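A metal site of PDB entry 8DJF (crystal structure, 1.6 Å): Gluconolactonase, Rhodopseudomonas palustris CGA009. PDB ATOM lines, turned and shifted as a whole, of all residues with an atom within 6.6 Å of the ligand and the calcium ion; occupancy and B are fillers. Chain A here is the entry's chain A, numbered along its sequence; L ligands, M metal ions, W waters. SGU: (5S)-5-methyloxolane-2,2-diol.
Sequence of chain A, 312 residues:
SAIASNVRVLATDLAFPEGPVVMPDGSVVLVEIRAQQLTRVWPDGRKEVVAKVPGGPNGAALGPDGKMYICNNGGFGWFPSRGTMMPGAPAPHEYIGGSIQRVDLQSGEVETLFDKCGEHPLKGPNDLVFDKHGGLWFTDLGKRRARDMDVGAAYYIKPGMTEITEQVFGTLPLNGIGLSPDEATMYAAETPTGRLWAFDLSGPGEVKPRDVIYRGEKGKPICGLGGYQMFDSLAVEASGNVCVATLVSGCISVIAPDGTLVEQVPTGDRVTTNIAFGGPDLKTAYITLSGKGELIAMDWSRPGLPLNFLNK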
ATOM      1  N   PHE A  16      16.346 -29.339  19.613  1.00  0.00           N
ATOM      2  CA  PHE A  16      15.403 -28.643  18.749  1.00  0.00           C
ATOM      3  C   PHE A  16      15.609 -27.130  18.875  1.00  0.00           C
ATOM      4  O   PHE A  16      14.798 -26.419  19.496  1.00  0.00           O
ATOM      5  CB  PHE A  16      13.941 -29.023  19.020  1.00  0.00           C
ATOM      6  CG  PHE A  16      13.060 -28.844  17.809  1.00  0.00           C
ATOM      7  CD1 PHE A  16      12.509 -27.614  17.502  1.00  0.00           C
ATOM      8  CD2 PHE A  16      12.837 -29.901  16.936  1.00  0.00           C
ATOM      9  CE1 PHE A  16      11.751 -27.432  16.362  1.00  0.00           C
ATOM     10  CE2 PHE A  16      12.063 -29.734  15.793  1.00  0.00           C
ATOM     11  CZ  PHE A  16      11.511 -28.500  15.503  1.00  0.00           C
ATOM     12  N   PRO A  17      16.681 -26.616  18.294  1.00  0.00           N
ATOM     13  CA  PRO A  17      16.928 -25.176  18.354  1.00  0.00           C
ATOM     14  C   PRO A  17      15.878 -24.370  17.594  1.00  0.00           C
ATOM     15  O   PRO A  17      15.338 -24.812  16.570  1.00  0.00           O
ATOM     16  CB  PRO A  17      18.318 -25.016  17.707  1.00  0.00           C
ATOM     17  CG  PRO A  17      18.431 -26.226  16.787  1.00  0.00           C
ATOM     18  CD  PRO A  17      17.757 -27.339  17.581  1.00  0.00           C
ATOM     19  N   GLU A  18      15.622 -23.166  18.094  1.00  0.00           N
ATOM     20  CA  GLU A  18      14.677 -22.238  17.478  1.00  0.00           C
ATOM     21  C   GLU A  18      14.970 -20.832  18.038  1.00  0.00           C
ATOM     22  O   GLU A  18      15.851 -20.657  18.870  1.00  0.00           O
ATOM     23  CB  GLU A  18      13.232 -22.683  17.717  1.00  0.00           C
ATOM     24  CG  GLU A  18      12.443 -23.086  16.465  1.00  0.00           C
ATOM     25  CD  GLU A  18      11.720 -21.896  15.811  1.00  0.00           C
ATOM     26  OE1 GLU A  18      12.117 -20.747  16.046  1.00  0.00           O
ATOM     27  OE2 GLU A  18      10.742 -22.129  15.046  1.00  0.00           O
ATOM     28  N   GLY A  19      14.168 -19.858  17.584  1.00  0.00           N
ATOM     29  CA  GLY A  19      14.212 -18.483  18.056  1.00  0.00           C
ATOM     30  C   GLY A  19      15.586 -17.899  18.253  1.00  0.00           C
ATOM     31  O   GLY A  19      15.864 -17.350  19.316  1.00  0.00           O
ATOM     32  N   ILE A  33      13.634 -26.080  22.262  1.00  0.00           N
ATOM     33  CA  ILE A  33      12.262 -26.379  22.627  1.00  0.00           C
ATOM     34  C   ILE A  33      12.214 -27.662  23.443  1.00  0.00           C
ATOM     35  O   ILE A  33      11.498 -27.754  24.448  1.00  0.00           O
ATOM     36  CB  ILE A  33      11.367 -26.487  21.370  1.00  0.00           C
ATOM     37  CG1 ILE A  33      11.649 -25.344  20.409  1.00  0.00           C
ATOM     38  CG2 ILE A  33       9.918 -26.434  21.812  1.00  0.00           C
ATOM     39  CD1 ILE A  33      10.630 -25.234  19.279  1.00  0.00           C
ATOM     40  N   ASN A  58       9.562 -21.320  22.232  1.00  0.00           N
ATOM     41  CA  ASN A  58       9.460 -21.510  20.776  1.00  0.00           C
ATOM     42  C   ASN A  58      10.056 -20.368  19.952  1.00  0.00           C
ATOM     43  O   ASN A  58      10.535 -20.604  18.833  1.00  0.00           O
ATOM     44  CB  ASN A  58       7.959 -21.666  20.425  1.00  0.00           C
ATOM     45  CG  ASN A  58       7.663 -22.446  19.155  1.00  0.00           C
ATOM     46  OD1 ASN A  58       6.612 -23.080  19.065  1.00  0.00           O
ATOM     47  ND2 ASN A  58       8.551 -22.380  18.156  1.00  0.00           N
ATOM     48  N   GLY A  59      10.024 -19.140  20.453  1.00  0.00           N
ATOM     49  CA  GLY A  59      10.572 -18.016  19.739  1.00  0.00           C
ATOM     50  C   GLY A  59      11.028 -16.987  20.761  1.00  0.00           C
ATOM     51  O   GLY A  59      10.568 -16.992  21.907  1.00  0.00           O
ATOM     52  N   ASN A  73       4.914 -22.240  23.682  1.00  0.00           N
ATOM     53  CA  ASN A  73       3.777 -22.942  23.092  1.00  0.00           C
ATOM     54  C   ASN A  73       3.147 -23.937  24.048  1.00  0.00           C
ATOM     55  O   ASN A  73       2.190 -24.633  23.664  1.00  0.00           O
ATOM     56  CB  ASN A  73       4.219 -23.610  21.802  1.00  0.00           C
ATOM     57  CG  ASN A  73       5.142 -24.807  22.018  1.00  0.00           C
ATOM     58  OD1 ASN A  73       5.004 -25.606  22.953  1.00  0.00           O
ATOM     59  ND2 ASN A  73       6.065 -24.955  21.099  1.00  0.00           N
ATOM     60  N   PHE A  76       5.252 -29.655  23.547  1.00  0.00           N
ATOM     61  CA  PHE A  76       4.893 -30.614  22.508  1.00  0.00           C
ATOM     62  C   PHE A  76       5.055 -32.042  23.039  1.00  0.00           C
ATOM     63  O   PHE A  76       5.503 -32.257  24.180  1.00  0.00           O
ATOM     64  CB  PHE A  76       5.780 -30.445  21.271  1.00  0.00           C
ATOM     65  CG  PHE A  76       5.457 -29.254  20.417  1.00  0.00           C
ATOM     66  CD1 PHE A  76       4.148 -28.975  20.053  1.00  0.00           C
ATOM     67  CD2 PHE A  76       6.477 -28.400  19.986  1.00  0.00           C
ATOM     68  CE1 PHE A  76       3.850 -27.872  19.254  1.00  0.00           C
ATOM     69  CE2 PHE A  76       6.188 -27.295  19.199  1.00  0.00           C
ATOM     70  CZ  PHE A  76       4.874 -27.042  18.818  1.00  0.00           C
ATOM     71  N   TRP A  78       7.222 -35.396  21.930  1.00  0.00           N
ATOM     72  CA  TRP A  78       8.355 -35.724  21.071  1.00  0.00           C
ATOM     73  C   TRP A  78       8.496 -37.220  20.787  1.00  0.00           C
ATOM     74  O   TRP A  78       8.448 -38.039  21.697  1.00  0.00           O
ATOM     75  CB  TRP A  78       9.645 -35.174  21.720  1.00  0.00           C
ATOM     76  CG  TRP A  78       9.569 -33.676  22.010  1.00  0.00           C
ATOM     77  CD1 TRP A  78       9.111 -33.086  23.152  1.00  0.00           C
ATOM     78  CD2 TRP A  78       9.950 -32.617  21.121  1.00  0.00           C
ATOM     79  NE1 TRP A  78       9.187 -31.705  23.030  1.00  0.00           N
ATOM     80  CE2 TRP A  78       9.693 -31.401  21.797  1.00  0.00           C
ATOM     81  CE3 TRP A  78      10.487 -32.579  19.832  1.00  0.00           C
ATOM     82  CZ2 TRP A  78       9.962 -30.160  21.221  1.00  0.00           C
ATOM     83  CZ3 TRP A  78      10.743 -31.346  19.259  1.00  0.00           C
ATOM     84  CH2 TRP A  78      10.471 -30.155  19.952  1.00  0.00           C
ATOM     85  N   PRO A  87       8.798 -33.042  17.003  1.00  0.00           N
ATOM     86  CA  PRO A  87       7.632 -32.721  17.834  1.00  0.00           C
ATOM     87  C   PRO A  87       6.351 -33.288  17.236  1.00  0.00           C
ATOM     88  O   PRO A  87       6.280 -33.652  16.058  1.00  0.00           O
ATOM     89  CB  PRO A  87       7.609 -31.187  17.872  1.00  0.00           C
ATOM     90  CG  PRO A  87       8.273 -30.764  16.611  1.00  0.00           C
ATOM     91  CD  PRO A  87       9.292 -31.858  16.270  1.00  0.00           C
ATOM     92  N   ASN A 126       4.144 -18.833  19.010  1.00  0.00           N
ATOM     93  CA  ASN A 126       5.227 -19.390  18.199  1.00  0.00           C
ATOM     94  C   ASN A 126       6.418 -18.460  17.964  1.00  0.00           C
ATOM     95  O   ASN A 126       7.544 -18.789  18.339  1.00  0.00           O
ATOM     96  CB  ASN A 126       4.675 -19.872  16.846  1.00  0.00           C
ATOM     97  CG  ASN A 126       5.667 -20.748  16.134  1.00  0.00           C
ATOM     98  OD1 ASN A 126       6.735 -20.302  15.669  1.00  0.00           O
ATOM     99  ND2 ASN A 126       5.361 -22.042  16.081  1.00  0.00           N
ATOM    100  N   ASP A 127       6.189 -17.321  17.347  1.00  0.00           N
ATOM    101  CA  ASP A 127       7.278 -16.364  17.136  1.00  0.00           C
ATOM    102  C   ASP A 127       6.766 -14.939  17.288  1.00  0.00           C
ATOM    103  O   ASP A 127       5.572 -14.689  17.417  1.00  0.00           O
ATOM    104  CB  ASP A 127       7.928 -16.557  15.759  1.00  0.00           C
ATOM    105  CG  ASP A 127       9.473 -16.366  15.793  1.00  0.00           C
ATOM    106  OD1 ASP A 127      10.002 -15.703  16.771  1.00  0.00           O
ATOM    107  OD2 ASP A 127      10.113 -16.794  14.809  1.00  0.00           O
ATOM    108  N   THR A 139       2.676 -14.663  16.815  1.00  0.00           N
ATOM    109  CA  THR A 139       1.799 -15.651  16.203  1.00  0.00           C
ATOM    110  C   THR A 139       1.403 -16.729  17.197  1.00  0.00           C
ATOM    111  O   THR A 139       2.109 -17.005  18.158  1.00  0.00           O
ATOM    112  CB  THR A 139       2.486 -16.311  15.001  1.00  0.00           C
ATOM    113  OG1 THR A 139       3.741 -16.796  15.418  1.00  0.00           O
ATOM    114  CG2 THR A 139       2.550 -15.436  13.835  1.00  0.00           C
ATOM    115  N   LEU A 141       0.400 -20.658  16.622  1.00  0.00           N
ATOM    116  CA  LEU A 141       0.284 -21.825  15.769  1.00  0.00           C
ATOM    117  C   LEU A 141      -0.891 -22.709  16.141  1.00  0.00           C
ATOM    118  O   LEU A 141      -1.329 -23.539  15.315  1.00  0.00           O
ATOM    119  CB  LEU A 141       1.610 -22.594  15.874  1.00  0.00           C
ATOM    120  CG  LEU A 141       1.784 -23.739  14.885  1.00  0.00           C
ATOM    121  CD1 LEU A 141       2.181 -23.192  13.512  1.00  0.00           C
ATOM    122  CD2 LEU A 141       2.774 -24.748  15.372  1.00  0.00           C
ATOM    123  N   ASN A 175       3.097 -19.011  12.005  1.00  0.00           N
ATOM    124  CA  ASN A 175       4.400 -19.390  12.505  1.00  0.00           C
ATOM    125  C   ASN A 175       5.323 -18.178  12.459  1.00  0.00           C
ATOM    126  O   ASN A 175       5.373 -17.389  13.407  1.00  0.00           O
ATOM    127  CB  ASN A 175       4.921 -20.574  11.674  1.00  0.00           C
ATOM    128  CG  ASN A 175       5.967 -21.365  12.406  1.00  0.00           C
ATOM    129  OD1 ASN A 175       6.904 -20.772  12.944  1.00  0.00           O
ATOM    130  ND2 ASN A 175       5.820 -22.682  12.466  1.00  0.00           N
ATOM    131  N   GLY A 176       6.067 -17.994  11.385  1.00  0.00           N
ATOM    132  CA  GLY A 176       6.941 -16.832  11.315  1.00  0.00           C
ATOM    133  C   GLY A 176       6.157 -15.548  11.280  1.00  0.00           C
ATOM    134  O   GLY A 176       5.017 -15.486  10.819  1.00  0.00           O
ATOM    135  N   THR A 191       1.896 -22.202   8.085  1.00  0.00           N
ATOM    136  CA  THR A 191       2.789 -23.356   8.018  1.00  0.00           C
ATOM    137  C   THR A 191       2.386 -24.407   6.990  1.00  0.00           C
ATOM    138  O   THR A 191       3.180 -24.710   6.095  1.00  0.00           O
ATOM    139  CB  THR A 191       2.903 -23.988   9.406  1.00  0.00           C
ATOM    140  OG1 THR A 191       3.662 -23.115  10.246  1.00  0.00           O
ATOM    141  CG2 THR A 191       3.614 -25.292   9.357  1.00  0.00           C
ATOM    142  N   PHE A 231       6.061 -23.815   5.764  1.00  0.00           N
ATOM    143  CA  PHE A 231       6.801 -22.668   6.285  1.00  0.00           C
ATOM    144  C   PHE A 231       6.926 -22.734   7.795  1.00  0.00           C
ATOM    145  O   PHE A 231       5.983 -23.102   8.497  1.00  0.00           O
ATOM    146  CB  PHE A 231       6.114 -21.344   5.920  1.00  0.00           C
ATOM    147  CG  PHE A 231       6.422 -20.828   4.548  1.00  0.00           C
ATOM    148  CD1 PHE A 231       7.641 -21.106   3.927  1.00  0.00           C
ATOM    149  CD2 PHE A 231       5.539 -19.951   3.926  1.00  0.00           C
ATOM    150  CE1 PHE A 231       7.916 -20.602   2.688  1.00  0.00           C
ATOM    151  CE2 PHE A 231       5.834 -19.406   2.708  1.00  0.00           C
ATOM    152  CZ  PHE A 231       7.021 -19.715   2.082  1.00  0.00           C
ATOM    153  N   ASP A 232       8.069 -22.249   8.299  1.00  0.00           N
ATOM    154  CA  ASP A 232       8.290 -22.097   9.740  1.00  0.00           C
ATOM    155  C   ASP A 232       8.504 -20.613   9.991  1.00  0.00           C
ATOM    156  O   ASP A 232       7.642 -19.809   9.648  1.00  0.00           O
ATOM    157  CB  ASP A 232       9.434 -22.982  10.192  1.00  0.00           C
ATOM    158  CG  ASP A 232       9.362 -23.326  11.672  1.00  0.00           C
ATOM    159  OD1 ASP A 232       9.137 -22.398  12.510  1.00  0.00           O
ATOM    160  OD2 ASP A 232       9.561 -24.509  12.009  1.00  0.00           O
ATOM    161  N   SER A 233       9.607 -20.229  10.620  1.00  0.00           N
ATOM    162  CA  SER A 233       9.855 -18.838  11.030  1.00  0.00           C
ATOM    163  C   SER A 233      10.569 -18.048   9.938  1.00  0.00           C
ATOM    164  O   SER A 233      11.010 -18.590   8.939  1.00  0.00           O
ATOM    165  CB  SER A 233      10.628 -18.833  12.346  1.00  0.00           C
ATOM    166  OG  SER A 233       9.738 -19.078  13.417  1.00  0.00           O
ATOM    167  N   LEU A 234      10.777 -16.739  10.183  1.00  0.00           N
ATOM    168  CA  LEU A 234      11.253 -15.872   9.121  1.00  0.00           C
ATOM    169  C   LEU A 234      12.071 -14.709   9.679  1.00  0.00           C
ATOM    170  O   LEU A 234      12.103 -14.466  10.897  1.00  0.00           O
ATOM    171  CB  LEU A 234      10.083 -15.332   8.281  1.00  0.00           C
ATOM    172  CG  LEU A 234       9.063 -14.431   8.946  1.00  0.00           C
ATOM    173  CD1 LEU A 234       9.555 -12.977   9.057  1.00  0.00           C
ATOM    174  CD2 LEU A 234       7.719 -14.467   8.265  1.00  0.00           C
ATOM    175  N   LEU A 247      10.294 -25.884   5.489  1.00  0.00           N
ATOM    176  CA  LEU A 247      10.325 -27.258   5.888  1.00  0.00           C
ATOM    177  C   LEU A 247      10.043 -28.174   4.686  1.00  0.00           C
ATOM    178  O   LEU A 247       9.457 -27.746   3.689  1.00  0.00           O
ATOM    179  CB  LEU A 247       9.295 -27.501   6.970  1.00  0.00           C
ATOM    180  CG  LEU A 247       9.358 -26.648   8.223  1.00  0.00           C
ATOM    181  CD1 LEU A 247       7.991 -26.713   8.901  1.00  0.00           C
ATOM    182  CD2 LEU A 247      10.438 -27.164   9.104  1.00  0.00           C
ATOM    183  N   VAL A 271      14.144 -30.067   8.301  1.00  0.00           N
ATOM    184  CA  VAL A 271      13.526 -29.348   9.412  1.00  0.00           C
ATOM    185  C   VAL A 271      14.301 -28.059   9.704  1.00  0.00           C
ATOM    186  O   VAL A 271      14.831 -27.882  10.808  1.00  0.00           O
ATOM    187  CB  VAL A 271      13.475 -30.237  10.670  1.00  0.00           C
ATOM    188  CG1 VAL A 271      12.592 -29.625  11.741  1.00  0.00           C
ATOM    189  CG2 VAL A 271      12.953 -31.628  10.308  1.00  0.00           C
ATOM    190  N   THR A 273      14.122 -24.250  10.560  1.00  0.00           N
ATOM    191  CA  THR A 273      13.014 -23.668  11.294  1.00  0.00           C
ATOM    192  C   THR A 273      13.081 -22.153  11.431  1.00  0.00           C
ATOM    193  O   THR A 273      12.038 -21.515  11.536  1.00  0.00           O
ATOM    194  CB  THR A 273      12.936 -24.258  12.713  1.00  0.00           C
ATOM    195  OG1 THR A 273      14.213 -24.115  13.363  1.00  0.00           O
ATOM    196  CG2 THR A 273      12.563 -25.732  12.673  1.00  0.00           C
ATOM    197  N   ASN A 274      14.272 -21.550  11.446  1.00  0.00           N
ATOM    198  CA  ASN A 274      14.319 -20.118  11.697  1.00  0.00           C
ATOM    199  C   ASN A 274      15.619 -19.554  11.133  1.00  0.00           C
ATOM    200  O   ASN A 274      16.577 -20.285  10.855  1.00  0.00           O
ATOM    201  CB  ASN A 274      14.150 -19.787  13.208  1.00  0.00           C
ATOM    202  CG  ASN A 274      13.435 -18.453  13.476  1.00  0.00           C
ATOM    203  OD1 ASN A 274      13.514 -17.490  12.687  1.00  0.00           O
ATOM    204  ND2 ASN A 274      12.689 -18.415  14.569  1.00  0.00           N
ATOM    205  N   SER A 290      16.804 -27.706  12.993  1.00  0.00           N
ATOM    206  CA  SER A 290      16.257 -28.364  14.172  1.00  0.00           C
ATOM    207  C   SER A 290      16.202 -29.872  14.033  1.00  0.00           C
ATOM    208  O   SER A 290      16.022 -30.566  15.044  1.00  0.00           O
ATOM    209  CB  SER A 290      14.884 -27.806  14.473  1.00  0.00           C
ATOM    210  OG  SER A 290      14.956 -26.411  14.751  1.00  0.00           O
HETATM  211  C02 SGU L   1       8.354 -24.737  15.085  1.00  0.00           C
HETATM  212  C04 SGU L   1       8.138 -25.436  16.417  1.00  0.00           C
HETATM  213  C05 SGU L   1       6.819 -26.187  16.212  1.00  0.00           C
HETATM  214  C06 SGU L   1       6.709 -26.378  14.691  1.00  0.00           C
HETATM  215  C07 SGU L   1       6.926 -27.789  14.180  1.00  0.00           C
HETATM  216  O01 SGU L   1       9.721 -24.669  14.727  1.00  0.00           O
HETATM  217  O03 SGU L   1       7.795 -23.495  15.138  1.00  0.00           O
HETATM  218  O08 SGU L   1       7.675 -25.482  14.103  1.00  0.00           O
HETATM  219 CA    CA M   1       8.640 -21.067  14.463  1.00  0.00          CA
HETATM  220  O   HOH W   1       9.441 -19.713  16.145  1.00  0.00           O
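Residues that only touch the calcium ion: Asn 58.
The nearest printed residue that does not touch the calcium ion is Thr 273 (4.5 Å).
O of Thr 273 sits at hydrogen-bond distance from N of Ser 233, at 2.9 Å.
The side-chain hydroxyl (OG) of Ser 233 lies close to the side-chain carboxylate (OD2) of Asp 127 (2.7 Å).
The backbone carbonyl oxygen (O) of Phe 16 lies within hydrogen-bond range of the backbone NH (N) of Ile 33 (3.0 Å).
The side-chain amide nitrogen of Asn 175 lies within hydrogen-bond range of the side-chain hydroxyl of Thr 191 (3.1 Å).
O of Asn 126 sits at hydrogen-bond distance from N of Gly 59 (3.3 Å).
The side-chain hydroxyl (OG1) of Thr 139 is in hydrogen-bond range of the backbone carbonyl oxygen (O) of Asn 175, 2.7 Å away.
The side-chain hydroxyl (OG) of Ser 233 lies close to the side-chain amide nitrogen (ND2) of Asn 274 (3.2 Å).
ND2 of Asn 126 sits at hydrogen-bond distance from OD1 of Asn 58, at 3.4 Å.
ND2 of Asn 58 lies close to O03 of the ligand, at 3.3 Å.
The calcium ion is bound by water W1 (2.3 Å), OD1 of Asn 175 (2.3 Å), OD1 of Asn 126 (2.4 Å), OD1 of Asp 232 (2.4 Å), OE2 of Glu 18 (2.4 Å), OG of Ser 233 (2.5 Å) and O03 of the ligand (2.7 Å).
Merely in contact with the ligand: Phe 76 (3.2 Å), Thr 273 (3.7 Å), Phe 16 (3.8 Å) and Ile 33 (3.8 Å).
Hydrophobic or aromatic side chains that line the ligand: Phe 16, Ile 33 and Phe 76.
Within 4 Å of the ligand: Phe 16, Glu 18, Ile 33, Asn 58, Phe 76, Asn 126, Asn 175, Asp 232 and Thr 273.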
